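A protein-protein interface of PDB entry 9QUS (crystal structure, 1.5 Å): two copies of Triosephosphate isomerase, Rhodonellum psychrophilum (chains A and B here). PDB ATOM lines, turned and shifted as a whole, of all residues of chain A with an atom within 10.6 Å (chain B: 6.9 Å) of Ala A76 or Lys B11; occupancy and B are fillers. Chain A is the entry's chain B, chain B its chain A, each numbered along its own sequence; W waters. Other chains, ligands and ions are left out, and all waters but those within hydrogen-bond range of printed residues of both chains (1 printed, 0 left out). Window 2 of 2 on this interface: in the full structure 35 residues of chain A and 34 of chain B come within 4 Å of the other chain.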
ATOM      1  N   SER A  70     -33.314  -2.343   9.034  1.00  0.00           N
ATOM      2  CA  SER A  70     -32.284  -1.318   8.964  1.00  0.00           C
ATOM      3  C   SER A  70     -32.780  -0.016   9.577  1.00  0.00           C
ATOM      4  O   SER A  70     -33.983   0.254   9.632  1.00  0.00           O
ATOM      5  CB  SER A  70     -31.874  -1.086   7.509  1.00  0.00           C
ATOM      6  OG  SER A  70     -30.786  -0.187   7.413  1.00  0.00           O
ATOM      7  N   ASP A  71     -31.835   0.790  10.065  1.00  0.00           N
ATOM      8  CA  ASP A  71     -32.150   2.153  10.466  1.00  0.00           C
ATOM      9  C   ASP A  71     -32.168   3.106   9.277  1.00  0.00           C
ATOM     10  O   ASP A  71     -32.542   4.273   9.443  1.00  0.00           O
ATOM     11  CB  ASP A  71     -31.152   2.648  11.521  1.00  0.00           C
ATOM     12  CG  ASP A  71     -29.729   2.697  11.010  1.00  0.00           C
ATOM     13  OD1 ASP A  71     -29.299   1.732  10.347  1.00  0.00           O
ATOM     14  OD2 ASP A  71     -29.038   3.701  11.281  1.00  0.00           O
ATOM     15  N   LYS A  72     -31.779   2.636   8.095  1.00  0.00           N
ATOM     16  CA  LYS A  72     -31.773   3.427   6.874  1.00  0.00           C
ATOM     17  C   LYS A  72     -32.987   3.079   6.019  1.00  0.00           C
ATOM     18  O   LYS A  72     -33.556   1.989   6.117  1.00  0.00           O
ATOM     19  CB  LYS A  72     -30.484   3.186   6.079  1.00  0.00           C
ATOM     20  CG  LYS A  72     -29.209   3.444   6.867  1.00  0.00           C
ATOM     21  CD  LYS A  72     -29.007   4.930   7.106  1.00  0.00           C
ATOM     22  CE  LYS A  72     -27.956   5.182   8.175  1.00  0.00           C
ATOM     23  NZ  LYS A  72     -27.830   6.636   8.489  1.00  0.00           N
ATOM     24  N   THR A  73     -33.382   4.030   5.169  1.00  0.00           N
ATOM     25  CA  THR A  73     -34.518   3.798   4.281  1.00  0.00           C
ATOM     26  C   THR A  73     -34.153   2.864   3.135  1.00  0.00           C
ATOM     27  O   THR A  73     -34.925   1.960   2.795  1.00  0.00           O
ATOM     28  CB  THR A  73     -35.034   5.121   3.712  1.00  0.00           C
ATOM     29  OG1 THR A  73     -33.934   5.879   3.191  1.00  0.00           O
ATOM     30  CG2 THR A  73     -35.761   5.926   4.775  1.00  0.00           C
ATOM     31  N   SER A  74     -32.985   3.068   2.530  1.00  0.00           N
ATOM     32  CA  SER A  74     -32.569   2.331   1.345  1.00  0.00           C
ATOM     33  C   SER A  74     -31.159   2.777   0.994  1.00  0.00           C
ATOM     34  O   SER A  74     -30.685   3.811   1.474  1.00  0.00           O
ATOM     35  CB  SER A  74     -33.503   2.578   0.161  1.00  0.00           C
ATOM     36  OG  SER A  74     -33.446   3.932  -0.257  1.00  0.00           O
ATOM     37  N   GLY A  75     -30.491   1.980   0.162  1.00  0.00           N
ATOM     38  CA  GLY A  75     -29.210   2.392  -0.373  1.00  0.00           C
ATOM     39  C   GLY A  75     -28.099   1.368  -0.313  1.00  0.00           C
ATOM     40  O   GLY A  75     -28.337   0.158  -0.393  1.00  0.00           O
ATOM     41  N   ALA A  76     -26.870   1.863  -0.160  1.00  0.00           N
ATOM     42  CA  ALA A  76     -25.669   1.035  -0.271  1.00  0.00           C
ATOM     43  C   ALA A  76     -25.368   0.366   1.069  1.00  0.00           C
ATOM     44  O   ALA A  76     -24.392   0.666   1.760  1.00  0.00           O
ATOM     45  CB  ALA A  76     -24.495   1.876  -0.752  1.00  0.00           C
ATOM     46  N   TYR A  77     -26.221  -0.593   1.416  1.00  0.00           N
ATOM     47  CA  TYR A  77     -26.111  -1.336   2.667  1.00  0.00           C
ATOM     48  C   TYR A  77     -26.314  -2.820   2.352  1.00  0.00           C
ATOM     49  O   TYR A  77     -27.303  -3.439   2.756  1.00  0.00           O
ATOM     50  CB  TYR A  77     -27.109  -0.815   3.696  1.00  0.00           C
ATOM     51  CG  TYR A  77     -27.018   0.683   3.876  1.00  0.00           C
ATOM     52  CD1 TYR A  77     -25.911   1.260   4.483  1.00  0.00           C
ATOM     53  CD2 TYR A  77     -28.016   1.524   3.403  1.00  0.00           C
ATOM     54  CE1 TYR A  77     -25.812   2.631   4.639  1.00  0.00           C
ATOM     55  CE2 TYR A  77     -27.927   2.899   3.557  1.00  0.00           C
ATOM     56  CZ  TYR A  77     -26.823   3.443   4.176  1.00  0.00           C
ATOM     57  OH  TYR A  77     -26.728   4.804   4.330  1.00  0.00           O
ATOM     58  N   THR A  78     -25.355  -3.376   1.613  1.00  0.00           N
ATOM     59  CA  THR A  78     -25.413  -4.771   1.202  1.00  0.00           C
ATOM     60  C   THR A  78     -25.698  -5.675   2.393  1.00  0.00           C
ATOM     61  O   THR A  78     -25.074  -5.553   3.452  1.00  0.00           O
ATOM     62  CB  THR A  78     -24.093  -5.166   0.534  1.00  0.00           C
ATOM     63  OG1 THR A  78     -23.887  -4.352  -0.629  1.00  0.00           O
ATOM     64  CG2 THR A  78     -24.099  -6.628   0.133  1.00  0.00           C
ATOM     65  N   GLY A  79     -26.658  -6.581   2.215  1.00  0.00           N
ATOM     66  CA  GLY A  79     -27.009  -7.545   3.233  1.00  0.00           C
ATOM     67  C   GLY A  79     -28.096  -7.109   4.193  1.00  0.00           C
ATOM     68  O   GLY A  79     -28.561  -7.934   4.991  1.00  0.00           O
ATOM     69  N   GLU A  80     -28.519  -5.853   4.138  1.00  0.00           N
ATOM     70  CA  GLU A  80     -29.487  -5.302   5.072  1.00  0.00           C
ATOM     71  C   GLU A  80     -30.876  -5.254   4.448  1.00  0.00           C
ATOM     72  O   GLU A  80     -31.040  -5.230   3.225  1.00  0.00           O
ATOM     73  CB  GLU A  80     -29.058  -3.901   5.515  1.00  0.00           C
ATOM     74  CG  GLU A  80     -27.745  -3.896   6.273  1.00  0.00           C
ATOM     75  CD  GLU A  80     -27.822  -4.703   7.554  1.00  0.00           C
ATOM     76  OE1 GLU A  80     -28.369  -4.189   8.551  1.00  0.00           O
ATOM     77  OE2 GLU A  80     -27.345  -5.857   7.557  1.00  0.00           O
ATOM     78  N   ILE A  81     -31.882  -5.236   5.321  1.00  0.00           N
ATOM     79  CA  ILE A  81     -33.288  -5.253   4.936  1.00  0.00           C
ATOM     80  C   ILE A  81     -33.945  -4.011   5.520  1.00  0.00           C
ATOM     81  O   ILE A  81     -33.799  -3.734   6.716  1.00  0.00           O
ATOM     82  CB  ILE A  81     -33.998  -6.529   5.429  1.00  0.00           C
ATOM     83  CG1 ILE A  81     -33.303  -7.776   4.873  1.00  0.00           C
ATOM     84  CG2 ILE A  81     -35.474  -6.502   5.038  1.00  0.00           C
ATOM     85  CD1 ILE A  81     -33.364  -7.901   3.364  1.00  0.00           C
ATOM     86  N   SER A  82     -34.667  -3.271   4.685  1.00  0.00           N
ATOM     87  CA  SER A  82     -35.294  -2.033   5.124  1.00  0.00           C
ATOM     88  C   SER A  82     -36.724  -2.285   5.593  1.00  0.00           C
ATOM     89  O   SER A  82     -37.356  -3.285   5.246  1.00  0.00           O
ATOM     90  CB  SER A  82     -35.296  -0.996   4.002  1.00  0.00           C
ATOM     91  OG  SER A  82     -36.216  -1.353   2.990  1.00  0.00           O
ATOM     92  N   SER A  84     -39.332  -0.593   4.693  1.00  0.00           N
ATOM     93  CA  SER A  84     -40.215  -0.547   3.532  1.00  0.00           C
ATOM     94  C   SER A  84     -40.280  -1.900   2.835  1.00  0.00           C
ATOM     95  O   SER A  84     -41.339  -2.300   2.338  1.00  0.00           O
ATOM     96  CB  SER A  84     -39.749   0.539   2.563  1.00  0.00           C
ATOM     97  OG  SER A  84     -38.369   0.416   2.280  1.00  0.00           O
ATOM     98  N   MET A  85     -39.157  -2.619   2.786  1.00  0.00           N
ATOM     99  CA  MET A  85     -39.172  -3.969   2.232  1.00  0.00           C
ATOM    100  C   MET A  85     -40.084  -4.877   3.047  1.00  0.00           C
ATOM    101  O   MET A  85     -40.894  -5.626   2.490  1.00  0.00           O
ATOM    102  CB  MET A  85     -37.755  -4.544   2.197  1.00  0.00           C
ATOM    103  CG  MET A  85     -36.805  -3.882   1.221  1.00  0.00           C
ATOM    104  SD  MET A  85     -35.176  -4.662   1.291  1.00  0.00           S
ATOM    105  CE  MET A  85     -34.265  -3.673   0.114  1.00  0.00           C
ATOM    106  N   GLY B   8     -25.300  -9.325 -10.126  1.00  0.00           N
ATOM    107  CA  GLY B   8     -25.939  -8.072  -9.773  1.00  0.00           C
ATOM    108  C   GLY B   8     -26.303  -7.954  -8.304  1.00  0.00           C
ATOM    109  O   GLY B   8     -27.177  -8.671  -7.804  1.00  0.00           O
ATOM    110  N   ASN B   9     -25.630  -7.047  -7.597  1.00  0.00           N
ATOM    111  CA  ASN B   9     -25.844  -6.831  -6.165  1.00  0.00           C
ATOM    112  C   ASN B   9     -26.809  -5.659  -5.995  1.00  0.00           C
ATOM    113  O   ASN B   9     -26.425  -4.494  -6.129  1.00  0.00           O
ATOM    114  CB  ASN B   9     -24.517  -6.581  -5.452  1.00  0.00           C
ATOM    115  CG  ASN B   9     -24.700  -6.196  -3.993  1.00  0.00           C
ATOM    116  OD1 ASN B   9     -25.756  -6.428  -3.404  1.00  0.00           O
ATOM    117  ND2 ASN B   9     -23.671  -5.601  -3.407  1.00  0.00           N
ATOM    118  N   TRP B  10     -28.069  -5.969  -5.683  1.00  0.00           N
ATOM    119  CA  TRP B  10     -29.057  -4.911  -5.500  1.00  0.00           C
ATOM    120  C   TRP B  10     -28.767  -4.056  -4.269  1.00  0.00           C
ATOM    121  O   TRP B  10     -29.342  -2.969  -4.134  1.00  0.00           O
ATOM    122  CB  TRP B  10     -30.470  -5.489  -5.359  1.00  0.00           C
ATOM    123  CG  TRP B  10     -30.951  -6.333  -6.487  1.00  0.00           C
ATOM    124  CD1 TRP B  10     -30.241  -6.733  -7.577  1.00  0.00           C
ATOM    125  CD2 TRP B  10     -32.267  -6.879  -6.638  1.00  0.00           C
ATOM    126  NE1 TRP B  10     -31.028  -7.505  -8.396  1.00  0.00           N
ATOM    127  CE2 TRP B  10     -32.279  -7.605  -7.845  1.00  0.00           C
ATOM    128  CE3 TRP B  10     -33.435  -6.822  -5.871  1.00  0.00           C
ATOM    129  CZ2 TRP B  10     -33.412  -8.274  -8.301  1.00  0.00           C
ATOM    130  CZ3 TRP B  10     -34.559  -7.484  -6.323  1.00  0.00           C
ATOM    131  CH2 TRP B  10     -34.541  -8.201  -7.530  1.00  0.00           C
ATOM    132  N   LYS B  11     -27.921  -4.532  -3.366  1.00  0.00           N
ATOM    133  CA  LYS B  11     -27.733  -3.890  -2.062  1.00  0.00           C
ATOM    134  C   LYS B  11     -29.115  -3.784  -1.413  1.00  0.00           C
ATOM    135  O   LYS B  11     -30.011  -4.581  -1.710  1.00  0.00           O
ATOM    136  CB  LYS B  11     -27.003  -2.575  -2.234  1.00  0.00           C
ATOM    137  CG  LYS B  11     -25.711  -2.694  -3.031  1.00  0.00           C
ATOM    138  CD  LYS B  11     -24.848  -1.446  -2.887  1.00  0.00           C
ATOM    139  CE  LYS B  11     -23.559  -1.578  -3.686  1.00  0.00           C
ATOM    140  NZ  LYS B  11     -22.675  -0.387  -3.531  1.00  0.00           N
ATOM    141  N   MET B  12     -29.312  -2.807  -0.527  1.00  0.00           N
ATOM    142  CA  MET B  12     -30.589  -2.650   0.170  1.00  0.00           C
ATOM    143  C   MET B  12     -31.508  -1.746  -0.653  1.00  0.00           C
ATOM    144  O   MET B  12     -31.772  -0.590  -0.319  1.00  0.00           O
ATOM    145  CB  MET B  12     -30.371  -2.097   1.572  1.00  0.00           C
ATOM    146  CG  MET B  12     -31.653  -1.961   2.363  1.00  0.00           C
ATOM    147  SD  MET B  12     -31.384  -1.606   4.112  1.00  0.00           S
ATOM    148  CE  MET B  12     -31.503   0.176   4.128  1.00  0.00           C
ATOM    149  N   ASN B  13     -31.999  -2.306  -1.755  1.00  0.00           N
ATOM    150  CA  ASN B  13     -32.860  -1.574  -2.669  1.00  0.00           C
ATOM    151  C   ASN B  13     -33.983  -2.474  -3.157  1.00  0.00           C
ATOM    152  O   ASN B  13     -33.792  -3.684  -3.309  1.00  0.00           O
ATOM    153  CB  ASN B  13     -32.067  -1.037  -3.870  1.00  0.00           C
ATOM    154  CG  ASN B  13     -31.088   0.054  -3.479  1.00  0.00           C
ATOM    155  OD1 ASN B  13     -31.475   1.208  -3.285  1.00  0.00           O
ATOM    156  ND2 ASN B  13     -29.812  -0.303  -3.371  1.00  0.00           N
ATOM    157  N   LEU B  14     -35.154  -1.864  -3.366  1.00  0.00           N
ATOM    158  CA  LEU B  14     -36.284  -2.460  -4.070  1.00  0.00           C
ATOM    159  C   LEU B  14     -37.227  -3.220  -3.151  1.00  0.00           C
ATOM    160  O   LEU B  14     -36.799  -4.087  -2.383  1.00  0.00           O
ATOM    161  CB  LEU B  14     -35.788  -3.394  -5.175  1.00  0.00           C
ATOM    162  CG  LEU B  14     -34.850  -2.794  -6.224  1.00  0.00           C
ATOM    163  CD1 LEU B  14     -34.792  -3.679  -7.465  1.00  0.00           C
ATOM    164  CD2 LEU B  14     -35.286  -1.379  -6.591  1.00  0.00           C
ATOM    165  N   ASN B  43     -28.334 -11.032  -6.975  1.00  0.00           N
ATOM    166  CA  ASN B  43     -28.207 -11.075  -5.524  1.00  0.00           C
ATOM    167  C   ASN B  43     -29.170 -10.070  -4.909  1.00  0.00           C
ATOM    168  O   ASN B  43     -28.753  -8.968  -4.532  1.00  0.00           O
ATOM    169  CB  ASN B  43     -26.773 -10.770  -5.088  1.00  0.00           C
ATOM    170  CG  ASN B  43     -25.770 -11.750  -5.668  1.00  0.00           C
ATOM    171  OD1 ASN B  43     -25.492 -12.794  -5.080  1.00  0.00           O
ATOM    172  ND2 ASN B  43     -25.216 -11.413  -6.827  1.00  0.00           N
ATOM    173  N   PRO B  44     -30.456 -10.396  -4.807  1.00  0.00           N
ATOM    174  CA  PRO B  44     -31.404  -9.465  -4.193  1.00  0.00           C
ATOM    175  C   PRO B  44     -31.362  -9.584  -2.680  1.00  0.00           C
ATOM    176  O   PRO B  44     -30.721 -10.496  -2.137  1.00  0.00           O
ATOM    177  CB  PRO B  44     -32.759  -9.925  -4.747  1.00  0.00           C
ATOM    178  CG  PRO B  44     -32.584 -11.422  -4.837  1.00  0.00           C
ATOM    179  CD  PRO B  44     -31.118 -11.647  -5.231  1.00  0.00           C
ATOM    180  N   PRO B  45     -32.041  -8.686  -1.972  1.00  0.00           N
ATOM    181  CA  PRO B  45     -32.172  -8.848  -0.518  1.00  0.00           C
ATOM    182  C   PRO B  45     -32.809 -10.185  -0.167  1.00  0.00           C
ATOM    183  O   PRO B  45     -33.445 -10.843  -0.995  1.00  0.00           O
ATOM    184  CB  PRO B  45     -33.068  -7.672  -0.106  1.00  0.00           C
ATOM    185  CG  PRO B  45     -32.869  -6.646  -1.192  1.00  0.00           C
ATOM    186  CD  PRO B  45     -32.647  -7.435  -2.461  1.00  0.00           C
ATOM    187  N   GLN B  67     -26.781 -11.659  -0.580  1.00  0.00           N
ATOM    188  CA  GLN B  67     -25.831 -10.601  -0.264  1.00  0.00           C
ATOM    189  C   GLN B  67     -25.022 -10.857   1.000  1.00  0.00           C
ATOM    190  O   GLN B  67     -24.101 -10.085   1.288  1.00  0.00           O
ATOM    191  CB  GLN B  67     -26.566  -9.262  -0.132  1.00  0.00           C
ATOM    192  CG  GLN B  67     -27.185  -8.789  -1.438  1.00  0.00           C
ATOM    193  CD  GLN B  67     -27.884  -7.445  -1.317  1.00  0.00           C
ATOM    194  OE1 GLN B  67     -27.623  -6.672  -0.395  1.00  0.00           O
ATOM    195  NE2 GLN B  67     -28.785  -7.165  -2.251  1.00  0.00           N
ATOM    196  N   HIS B  98     -18.421  -8.221   1.544  1.00  0.00           N
ATOM    197  CA  HIS B  98     -18.592  -6.971   0.815  1.00  0.00           C
ATOM    198  C   HIS B  98     -18.071  -5.797   1.641  1.00  0.00           C
ATOM    199  O   HIS B  98     -18.155  -5.784   2.874  1.00  0.00           O
ATOM    200  CB  HIS B  98     -20.067  -6.764   0.460  1.00  0.00           C
ATOM    201  CG  HIS B  98     -20.302  -5.691  -0.559  1.00  0.00           C
ATOM    202  ND1 HIS B  98     -20.439  -4.363  -0.222  1.00  0.00           N
ATOM    203  CD2 HIS B  98     -20.434  -5.752  -1.906  1.00  0.00           C
ATOM    204  CE1 HIS B  98     -20.638  -3.649  -1.315  1.00  0.00           C
ATOM    205  NE2 HIS B  98     -20.640  -4.469  -2.352  1.00  0.00           N
ATOM    206  N   SER B  99     -17.527  -4.800   0.943  1.00  0.00           N
ATOM    207  CA  SER B  99     -16.898  -3.675   1.628  1.00  0.00           C
ATOM    208  C   SER B  99     -17.868  -2.986   2.579  1.00  0.00           C
ATOM    209  O   SER B  99     -17.469  -2.516   3.651  1.00  0.00           O
ATOM    210  CB  SER B  99     -16.361  -2.672   0.605  1.00  0.00           C
ATOM    211  OG  SER B  99     -17.405  -2.169  -0.212  1.00  0.00           O
ATOM    212  N   GLU B 100     -19.144  -2.901   2.196  1.00  0.00           N
ATOM    213  CA  GLU B 100     -20.135  -2.221   3.022  1.00  0.00           C
ATOM    214  C   GLU B 100     -20.445  -2.975   4.306  1.00  0.00           C
ATOM    215  O   GLU B 100     -20.863  -2.353   5.284  1.00  0.00           O
ATOM    216  CB  GLU B 100     -21.411  -1.998   2.207  1.00  0.00           C
ATOM    217  CG  GLU B 100     -21.205  -1.069   1.013  1.00  0.00           C
ATOM    218  CD  GLU B 100     -22.298  -1.191  -0.040  1.00  0.00           C
ATOM    219  OE1 GLU B 100     -23.286  -1.924   0.191  1.00  0.00           O
ATOM    220  OE2 GLU B 100     -22.157  -0.555  -1.108  1.00  0.00           O
ATOM    221  N   GLU B 103     -17.311  -2.491   6.585  1.00  0.00           N
ATOM    222  CA  GLU B 103     -17.321  -1.159   7.180  1.00  0.00           C
ATOM    223  C   GLU B 103     -18.386  -1.038   8.261  1.00  0.00           C
ATOM    224  O   GLU B 103     -18.070  -0.843   9.436  1.00  0.00           O
ATOM    225  CB  GLU B 103     -17.554  -0.108   6.096  1.00  0.00           C
ATOM    226  CG  GLU B 103     -17.670   1.319   6.613  1.00  0.00           C
ATOM    227  CD  GLU B 103     -17.793   2.345   5.499  1.00  0.00           C
ATOM    228  OE1 GLU B 103     -18.492   2.070   4.503  1.00  0.00           O
ATOM    229  OE2 GLU B 103     -17.179   3.424   5.616  1.00  0.00           O
ATOM    230  N   TYR B 104     -19.655  -1.181   7.880  1.00  0.00           N
ATOM    231  CA  TYR B 104     -20.753  -0.865   8.786  1.00  0.00           C
ATOM    232  C   TYR B 104     -20.982  -1.921   9.857  1.00  0.00           C
ATOM    233  O   TYR B 104     -21.543  -1.598  10.912  1.00  0.00           O
ATOM    234  CB  TYR B 104     -22.035  -0.664   7.981  1.00  0.00           C
ATOM    235  CG  TYR B 104     -21.976   0.546   7.084  1.00  0.00           C
ATOM    236  CD1 TYR B 104     -21.417   0.469   5.817  1.00  0.00           C
ATOM    237  CD2 TYR B 104     -22.445   1.777   7.519  1.00  0.00           C
ATOM    238  CE1 TYR B 104     -21.351   1.582   4.996  1.00  0.00           C
ATOM    239  CE2 TYR B 104     -22.385   2.890   6.711  1.00  0.00           C
ATOM    240  CZ  TYR B 104     -21.839   2.789   5.450  1.00  0.00           C
ATOM    241  OH  TYR B 104     -21.776   3.898   4.642  1.00  0.00           O
ATOM    242  N   GLU B 170     -13.110  -4.985  -5.050  1.00  0.00           N
ATOM    243  CA  GLU B 170     -13.769  -3.701  -4.884  1.00  0.00           C
ATOM    244  C   GLU B 170     -12.713  -2.611  -4.770  1.00  0.00           C
ATOM    245  O   GLU B 170     -12.039  -2.530  -3.733  1.00  0.00           O
ATOM    246  CB  GLU B 170     -14.662  -3.701  -3.644  1.00  0.00           C
ATOM    247  CG  GLU B 170     -15.764  -4.746  -3.633  1.00  0.00           C
ATOM    248  CD  GLU B 170     -16.730  -4.540  -2.488  1.00  0.00           C
ATOM    249  OE1 GLU B 170     -17.462  -3.529  -2.503  1.00  0.00           O
ATOM    250  OE2 GLU B 170     -16.751  -5.381  -1.569  1.00  0.00           O
ATOM    251  N   ILE B 175     -14.424   4.410  -5.347  1.00  0.00           N
ATOM    252  CA  ILE B 175     -15.879   4.337  -5.282  1.00  0.00           C
ATOM    253  C   ILE B 175     -16.343   5.499  -4.414  1.00  0.00           C
ATOM    254  O   ILE B 175     -16.270   5.437  -3.181  1.00  0.00           O
ATOM    255  CB  ILE B 175     -16.367   2.993  -4.732  1.00  0.00           C
ATOM    256  CG1 ILE B 175     -16.072   1.885  -5.743  1.00  0.00           C
ATOM    257  CG2 ILE B 175     -17.855   3.059  -4.418  1.00  0.00           C
ATOM    258  CD1 ILE B 175     -16.037   0.495  -5.146  1.00  0.00           C
ATOM    259  N   ILE B 236     -21.772  -6.045  -9.982  1.00  0.00           N
ATOM    260  CA  ILE B 236     -22.359  -4.791 -10.437  1.00  0.00           C
ATOM    261  C   ILE B 236     -23.175  -4.151  -9.324  1.00  0.00           C
ATOM    262  O   ILE B 236     -23.950  -4.821  -8.627  1.00  0.00           O
ATOM    263  CB  ILE B 236     -23.221  -5.024 -11.690  1.00  0.00           C
ATOM    264  CG1 ILE B 236     -22.393  -5.700 -12.783  1.00  0.00           C
ATOM    265  CG2 ILE B 236     -23.797  -3.708 -12.194  1.00  0.00           C
ATOM    266  CD1 ILE B 236     -23.207  -6.153 -13.961  1.00  0.00           C
ATOM    267  N   GLY B 237     -23.025  -2.839  -9.182  1.00  0.00           N
ATOM    268  CA  GLY B 237     -23.810  -2.088  -8.228  1.00  0.00           C
ATOM    269  C   GLY B 237     -25.082  -1.525  -8.825  1.00  0.00           C
ATOM    270  O   GLY B 237     -25.978  -2.275  -9.220  1.00  0.00           O
ATOM    271  N   GLY B 238     -25.155  -0.197  -8.920  1.00  0.00           N
ATOM    272  CA  GLY B 238     -26.402   0.452  -9.284  1.00  0.00           C
ATOM    273  C   GLY B 238     -27.009  -0.041 -10.583  1.00  0.00           C
ATOM    274  O   GLY B 238     -28.234  -0.069 -10.725  1.00  0.00           O
ATOM    275  N   SER B 240     -27.320  -2.896 -11.545  1.00  0.00           N
ATOM    276  CA  SER B 240     -28.143  -4.068 -11.274  1.00  0.00           C
ATOM    277  C   SER B 240     -29.623  -3.720 -11.288  1.00  0.00           C
ATOM    278  O   SER B 240     -30.457  -4.557 -11.659  1.00  0.00           O
ATOM    279  CB  SER B 240     -27.772  -4.669  -9.916  1.00  0.00           C
ATOM    280  OG  SER B 240     -26.425  -5.098  -9.882  1.00  0.00           O
ATOM    281  N   LEU B 241     -29.971  -2.494 -10.894  1.00  0.00           N
ATOM    282  CA  LEU B 241     -31.361  -2.112 -10.703  1.00  0.00           C
ATOM    283  C   LEU B 241     -32.045  -1.646 -11.982  1.00  0.00           C
ATOM    284  O   LEU B 241     -33.251  -1.379 -11.952  1.00  0.00           O
ATOM    285  CB  LEU B 241     -31.449  -1.008  -9.646  1.00  0.00           C
ATOM    286  CG  LEU B 241     -30.680  -1.268  -8.346  1.00  0.00           C
ATOM    287  CD1 LEU B 241     -30.956  -0.176  -7.321  1.00  0.00           C
ATOM    288  CD2 LEU B 241     -31.026  -2.641  -7.785  1.00  0.00           C
HETATM  289  O   HOH W   1     -30.141  -6.845   1.425  1.00  0.00           O
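Water W1 bridges the backbone carbonyl oxygen (O) of Glu A80 and the side-chain amide oxygen (OE1) of Gln B67.
OG of Ser B240 is in hydrogen-bond range of N of Asn B9, at 3.1 Å.
NE2 of Gln B67 is in hydrogen-bond range of O of Lys B11.
The backbone NH (N) of Glu B100 lies within hydrogen-bond range of a ring nitrogen (ND1) of His B98 (3.1 Å).
OE1 of Glu B170 lies within hydrogen-bond range of NE2 of His B98, 3.3 Å away.
The backbone NH (N) of Ser A70 sits at hydrogen-bond distance from the backbone carbonyl oxygen (O) of Ile A81 (2.7 Å).
The side-chain hydroxyl (OG) of Ser A82 is in hydrogen-bond range of the side-chain hydroxyl (OG) of Ser A84.
Among the printed residues, pairs that only touch across the chains: Met A85 with Asn B13 (3.2 Å), Thr A78 with Gln B67 (3.3 Å), Lys A72 with Met B12 (3.4 Å), Thr A78 with Lys B11 (3.4 Å), Met A85 with Met B12 (3.5 Å), Ser A74 with Met B12 (3.5 Å), Ile A81 with Pro B45 (3.5 Å), Met A85 with Pro B45 (3.5 Å), Tyr A77 with Met B12 (3.6 Å), Gly A75 with Lys B11 (3.6 Å), Met A85 with Leu B14 (3.6 Å), Ala A76 with Lys B11 (3.7 Å), Ile A81 with Met B12 (3.8 Å) and Thr A73 with Met B12 (3.9 Å).
No position is printed for both chains.
Of the 25 pairs that touch across the chains among the printed residues, none has its exchanged pair printed and touching as well.
Of the 23 printed residues of chain B, 9 touch a printed residue of chain A.
Hydrophobic or aromatic side chains of chain B within 4 Å of the printed part of chain A: Met B12, Pro B45 and His B98.
Of the 15 printed residues of chain A, 13 touch a printed residue of chain B.
Hydrophobic or aromatic side chains of chain A within 4 Å of the printed part of chain B: Ala A76, Tyr A77, Ile A81 and Met A85.
Along chain A the printed residues that touch a printed residue of chain B span positions 70 to 85.
Among the printed residues, 25 pairs touch across the chains.
Among the printed residues, no Asp or Glu carboxylate lies within 4 Å of a Lys or Arg side-chain nitrogen of the other chain.
Of chain B, only Lys B11 (3.7 Å) and Glu B100 (3.2 Å) come within 4 Å of Ala A76.
Printed residues of chain A within 4 Å of Lys B11: Gly A75 (3.6 Å), Ala A76 (3.7 Å) and Thr A78 (3.4 Å).
Of chain A, only Thr A78 comes within 4 Å of Asn B9.
Met B12 touches ten residues of chain A.
Asn B13 touches just these residues of chain A: Gly A75 (3.4 Å) and Met A85 (3.2 Å).
Glu B100 touches just these residues of chain A: Ala A76 (3.2 Å), Tyr A77 (3.4 Å) and Thr A78 (2.6 Å).
No residue of chain A comes within 4 Å of Gly B237.
Of the printed residues of chain B, Ser A70 touches Met B12.
Of the printed residues of chain B, Thr A73 touches Met B12 (3.9 Å).
The nearest residue of chain B that does not touch Ala A76 is Tyr B104 (4.5 Å).
The nearest residue of chain A that does not touch Lys B11 is Tyr A77 (4.2 Å).
The side-chain hydroxyl of Thr A78 sits at hydrogen-bond distance from the side-chain amide nitrogen of Asn B9 (3.1 Å).
The side-chain sulfur (SD) of Met B12 sits close to the side-chain hydroxyl (OG) of Ser A70, 3.6 Å away.
The backbone NH of Gly A75 lies within hydrogen-bond range of the backbone carbonyl oxygen of Met B12 (2.9 Å).
N of Ser A82 is in hydrogen-bond range of SD of Met B12 (3.7 Å).
The side-chain amide nitrogen of Asn B13 is in hydrogen-bond range of the backbone carbonyl oxygen of Gly A75 (3.4 Å).
The side-chain amide oxygen (OE1) of Gln B67 sits at hydrogen-bond distance from the backbone NH (N) of Gly A79.
The side-chain hydroxyl of Thr A78 sits close to a ring nitrogen (ND1) of His B98 (3.5 Å).
The backbone NH (N) of Tyr A77 is in hydrogen-bond range of the side-chain carboxylate (OE1) of Glu B100.
The side-chain hydroxyl of Thr A78 lies within hydrogen-bond range of the side-chain carboxylate of Glu B100 (2.6 Å).
The side-chain carboxylate of Glu B100 sits close to the backbone carbonyl oxygen of Ala A76 (3.2 Å).
The backbone carbonyl oxygen (O) of Glu A80 lies close to the side-chain sulfur (SD) of Met B12, at 3.7 Å.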
